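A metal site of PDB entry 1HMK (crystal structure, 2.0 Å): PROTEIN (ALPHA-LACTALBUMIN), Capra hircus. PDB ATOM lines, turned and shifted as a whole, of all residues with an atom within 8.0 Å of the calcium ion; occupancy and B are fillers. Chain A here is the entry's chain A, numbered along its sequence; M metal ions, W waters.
Within 4 Å of the calcium ion: Lys 80, Asp 83, Asp 85, Asp 88 and Asp 89.
The nearest printed residue that does not touch the calcium ion is Phe 81 (4.1 Å).
Water W2 bridges OD2 of Asp 83 (2.6 Å) and OD2 of Asp 88 (2.6 Å).
The side-chain carboxylate of Asp 85 sits at hydrogen-bond distance from the side-chain hydroxyl of Thr 87 (2.6 Å).
The side-chain amino group (NZ) of Lys 80 lies within salt-bridge range of the side-chain carboxylate (OD2) of Asp 79.
The calcium ion is bound by O of Asp 85 (2.4 Å), OD1 of Asp 83 (2.4 Å), O of Lys 80 (2.4 Å), OD1 of Asp 89 (2.5 Å), OD1 of Asp 88 (2.5 Å), water W1 (2.5 Å) and water W2 (2.6 Å).
The calcium ion has seven donor atoms within binding distance.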
ATOM      1  N   THR A  39       5.968  -8.624  -6.728  1.00  0.00           N
ATOM      2  CA  THR A  39       7.347  -8.669  -6.238  1.00  0.00           C
ATOM      3  C   THR A  39       7.910  -7.289  -5.854  1.00  0.00           C
ATOM      4  O   THR A  39       9.020  -7.188  -5.325  1.00  0.00           O
ATOM      5  CB  THR A  39       8.304  -9.310  -7.263  1.00  0.00           C
ATOM      6  OG1 THR A  39       8.137  -8.672  -8.537  1.00  0.00           O
ATOM      7  CG2 THR A  39       8.029 -10.802  -7.395  1.00  0.00           C
ATOM      8  N   ILE A  76      20.973  -7.808   4.913  1.00  0.00           N
ATOM      9  CA  ILE A  76      20.801  -7.339   3.545  1.00  0.00           C
ATOM     10  C   ILE A  76      19.974  -6.044   3.497  1.00  0.00           C
ATOM     11  O   ILE A  76      19.273  -5.719   4.450  1.00  0.00           O
ATOM     12  CB  ILE A  76      20.083  -8.432   2.711  1.00  0.00           C
ATOM     13  CG1 ILE A  76      20.058  -8.055   1.224  1.00  0.00           C
ATOM     14  CG2 ILE A  76      18.666  -8.652   3.236  1.00  0.00           C
ATOM     15  CD1 ILE A  76      19.530  -9.153   0.336  1.00  0.00           C
ATOM     16  N   SER A  77      20.066  -5.303   2.400  1.00  0.00           N
ATOM     17  CA  SER A  77      19.278  -4.083   2.255  1.00  0.00           C
ATOM     18  C   SER A  77      17.900  -4.492   1.707  1.00  0.00           C
ATOM     19  O   SER A  77      17.806  -5.291   0.758  1.00  0.00           O
ATOM     20  CB  SER A  77      19.971  -3.091   1.312  1.00  0.00           C
ATOM     21  OG  SER A  77      20.070  -3.592  -0.010  1.00  0.00           O
ATOM     22  N   CYS A  78      16.850  -3.958   2.308  1.00  0.00           N
ATOM     23  CA  CYS A  78      15.472  -4.295   1.919  1.00  0.00           C
ATOM     24  C   CYS A  78      15.120  -4.136   0.458  1.00  0.00           C
ATOM     25  O   CYS A  78      14.261  -4.847  -0.060  1.00  0.00           O
ATOM     26  CB  CYS A  78      14.481  -3.487   2.757  1.00  0.00           C
ATOM     27  SG  CYS A  78      14.633  -3.683   4.552  1.00  0.00           S
ATOM     28  N   ASP A  79      15.755  -3.192  -0.215  1.00  0.00           N
ATOM     29  CA  ASP A  79      15.471  -2.944  -1.625  1.00  0.00           C
ATOM     30  C   ASP A  79      15.834  -4.143  -2.492  1.00  0.00           C
ATOM     31  O   ASP A  79      15.436  -4.223  -3.651  1.00  0.00           O
ATOM     32  CB  ASP A  79      16.244  -1.719  -2.105  1.00  0.00           C
ATOM     33  CG  ASP A  79      17.742  -1.962  -2.122  1.00  0.00           C
ATOM     34  OD1 ASP A  79      18.354  -1.987  -1.039  1.00  0.00           O
ATOM     35  OD2 ASP A  79      18.299  -2.127  -3.234  1.00  0.00           O
ATOM     36  N   LYS A  80      16.609  -5.058  -1.922  1.00  0.00           N
ATOM     37  CA  LYS A  80      17.001  -6.256  -2.647  1.00  0.00           C
ATOM     38  C   LYS A  80      15.804  -7.175  -2.788  1.00  0.00           C
ATOM     39  O   LYS A  80      15.840  -8.118  -3.567  1.00  0.00           O
ATOM     40  CB  LYS A  80      18.126  -6.973  -1.915  1.00  0.00           C
ATOM     41  CG  LYS A  80      19.415  -7.052  -2.707  1.00  0.00           C
ATOM     42  CD  LYS A  80      19.994  -5.668  -2.932  1.00  0.00           C
ATOM     43  CE  LYS A  80      19.780  -5.205  -4.361  1.00  0.00           C
ATOM     44  NZ  LYS A  80      19.632  -3.726  -4.447  1.00  0.00           N
ATOM     45  N   PHE A  81      14.738  -6.900  -2.037  1.00  0.00           N
ATOM     46  CA  PHE A  81      13.540  -7.724  -2.099  1.00  0.00           C
ATOM     47  C   PHE A  81      12.505  -7.087  -3.002  1.00  0.00           C
ATOM     48  O   PHE A  81      11.320  -7.445  -2.959  1.00  0.00           O
ATOM     49  CB  PHE A  81      12.956  -7.910  -0.701  1.00  0.00           C
ATOM     50  CG  PHE A  81      13.887  -8.571   0.279  1.00  0.00           C
ATOM     51  CD1 PHE A  81      14.682  -9.648  -0.120  1.00  0.00           C
ATOM     52  CD2 PHE A  81      13.959  -8.137   1.595  1.00  0.00           C
ATOM     53  CE1 PHE A  81      15.534 -10.280   0.786  1.00  0.00           C
ATOM     54  CE2 PHE A  81      14.805  -8.757   2.512  1.00  0.00           C
ATOM     55  CZ  PHE A  81      15.589  -9.836   2.101  1.00  0.00           C
ATOM     56  N   LEU A  82      12.931  -6.130  -3.812  1.00  0.00           N
ATOM     57  CA  LEU A  82      12.015  -5.445  -4.702  1.00  0.00           C
ATOM     58  C   LEU A  82      12.313  -5.730  -6.171  1.00  0.00           C
ATOM     59  O   LEU A  82      11.618  -5.224  -7.055  1.00  0.00           O
ATOM     60  CB  LEU A  82      12.056  -3.932  -4.451  1.00  0.00           C
ATOM     61  CG  LEU A  82      11.542  -3.456  -3.078  1.00  0.00           C
ATOM     62  CD1 LEU A  82      11.608  -1.922  -3.025  1.00  0.00           C
ATOM     63  CD2 LEU A  82      10.121  -3.942  -2.839  1.00  0.00           C
ATOM     64  N   ASP A  83      13.327  -6.542  -6.435  1.00  0.00           N
ATOM     65  CA  ASP A  83      13.682  -6.871  -7.816  1.00  0.00           C
ATOM     66  C   ASP A  83      13.103  -8.210  -8.269  1.00  0.00           C
ATOM     67  O   ASP A  83      12.352  -8.862  -7.539  1.00  0.00           O
ATOM     68  CB  ASP A  83      15.201  -6.867  -7.993  1.00  0.00           C
ATOM     69  CG  ASP A  83      15.898  -7.849  -7.089  1.00  0.00           C
ATOM     70  OD1 ASP A  83      15.239  -8.805  -6.651  1.00  0.00           O
ATOM     71  OD2 ASP A  83      17.105  -7.669  -6.805  1.00  0.00           O
ATOM     72  N   ASP A  84      13.464  -8.616  -9.476  1.00  0.00           N
ATOM     73  CA  ASP A  84      12.969  -9.857 -10.059  1.00  0.00           C
ATOM     74  C   ASP A  84      13.599 -11.130  -9.521  1.00  0.00           C
ATOM     75  O   ASP A  84      12.979 -12.189  -9.528  1.00  0.00           O
ATOM     76  CB  ASP A  84      13.135  -9.819 -11.584  1.00  0.00           C
ATOM     77  CG  ASP A  84      12.540  -8.562 -12.211  1.00  0.00           C
ATOM     78  OD1 ASP A  84      12.231  -7.600 -11.477  1.00  0.00           O
ATOM     79  OD2 ASP A  84      12.393  -8.528 -13.462  1.00  0.00           O
ATOM     80  N   ASP A  85      14.834 -11.044  -9.050  1.00  0.00           N
ATOM     81  CA  ASP A  85      15.534 -12.220  -8.531  1.00  0.00           C
ATOM     82  C   ASP A  85      15.108 -12.634  -7.128  1.00  0.00           C
ATOM     83  O   ASP A  85      15.604 -12.097  -6.148  1.00  0.00           O
ATOM     84  CB  ASP A  85      17.040 -11.964  -8.543  1.00  0.00           C
ATOM     85  CG  ASP A  85      17.858 -13.235  -8.399  1.00  0.00           C
ATOM     86  OD1 ASP A  85      17.281 -14.294  -8.086  1.00  0.00           O
ATOM     87  OD2 ASP A  85      19.081 -13.167  -8.609  1.00  0.00           O
ATOM     88  N   LEU A  86      14.208 -13.611  -7.017  1.00  0.00           N
ATOM     89  CA  LEU A  86      13.732 -14.052  -5.713  1.00  0.00           C
ATOM     90  C   LEU A  86      14.721 -14.912  -4.921  1.00  0.00           C
ATOM     91  O   LEU A  86      14.398 -15.393  -3.839  1.00  0.00           O
ATOM     92  CB  LEU A  86      12.414 -14.820  -5.864  1.00  0.00           C
ATOM     93  CG  LEU A  86      11.294 -14.025  -6.550  1.00  0.00           C
ATOM     94  CD1 LEU A  86      10.032 -14.860  -6.617  1.00  0.00           C
ATOM     95  CD2 LEU A  86      11.059 -12.725  -5.783  1.00  0.00           C
ATOM     96  N   THR A  87      15.932 -15.094  -5.457  1.00  0.00           N
ATOM     97  CA  THR A  87      16.938 -15.908  -4.778  1.00  0.00           C
ATOM     98  C   THR A  87      17.205 -15.473  -3.346  1.00  0.00           C
ATOM     99  O   THR A  87      17.147 -16.295  -2.433  1.00  0.00           O
ATOM    100  CB  THR A  87      18.285 -15.920  -5.545  1.00  0.00           C
ATOM    101  OG1 THR A  87      18.086 -16.474  -6.858  1.00  0.00           O
ATOM    102  CG2 THR A  87      19.315 -16.762  -4.814  1.00  0.00           C
ATOM    103  N   ASP A  88      17.491 -14.187  -3.132  1.00  0.00           N
ATOM    104  CA  ASP A  88      17.755 -13.715  -1.778  1.00  0.00           C
ATOM    105  C   ASP A  88      16.496 -13.612  -0.924  1.00  0.00           C
ATOM    106  O   ASP A  88      16.567 -13.784   0.297  1.00  0.00           O
ATOM    107  CB  ASP A  88      18.517 -12.374  -1.794  1.00  0.00           C
ATOM    108  CG  ASP A  88      17.986 -11.411  -2.822  1.00  0.00           C
ATOM    109  OD1 ASP A  88      16.814 -11.553  -3.216  1.00  0.00           O
ATOM    110  OD2 ASP A  88      18.743 -10.502  -3.236  1.00  0.00           O
ATOM    111  N   ASP A  89      15.346 -13.338  -1.541  1.00  0.00           N
ATOM    112  CA  ASP A  89      14.094 -13.265  -0.794  1.00  0.00           C
ATOM    113  C   ASP A  89      13.824 -14.637  -0.179  1.00  0.00           C
ATOM    114  O   ASP A  89      13.347 -14.753   0.943  1.00  0.00           O
ATOM    115  CB  ASP A  89      12.903 -12.920  -1.699  1.00  0.00           C
ATOM    116  CG  ASP A  89      13.130 -11.686  -2.525  1.00  0.00           C
ATOM    117  OD1 ASP A  89      14.231 -11.558  -3.073  1.00  0.00           O
ATOM    118  OD2 ASP A  89      12.207 -10.852  -2.623  1.00  0.00           O
ATOM    119  N   ILE A  90      14.126 -15.679  -0.948  1.00  0.00           N
ATOM    120  CA  ILE A  90      13.923 -17.049  -0.504  1.00  0.00           C
ATOM    121  C   ILE A  90      14.872 -17.404   0.637  1.00  0.00           C
ATOM    122  O   ILE A  90      14.470 -18.045   1.611  1.00  0.00           O
ATOM    123  CB  ILE A  90      14.109 -18.036  -1.694  1.00  0.00           C
ATOM    124  CG1 ILE A  90      12.867 -17.997  -2.581  1.00  0.00           C
ATOM    125  CG2 ILE A  90      14.323 -19.453  -1.178  1.00  0.00           C
ATOM    126  CD1 ILE A  90      12.974 -18.797  -3.859  1.00  0.00           C
HETATM  127 CA    CA M   1      15.401 -10.211  -4.753  1.00  0.00          CA
HETATM  128  O   HOH W   1      12.972  -9.567  -5.108  1.00  0.00           O
HETATM  129  O   HOH W   2      17.819  -9.877  -5.633  1.00  0.00           O
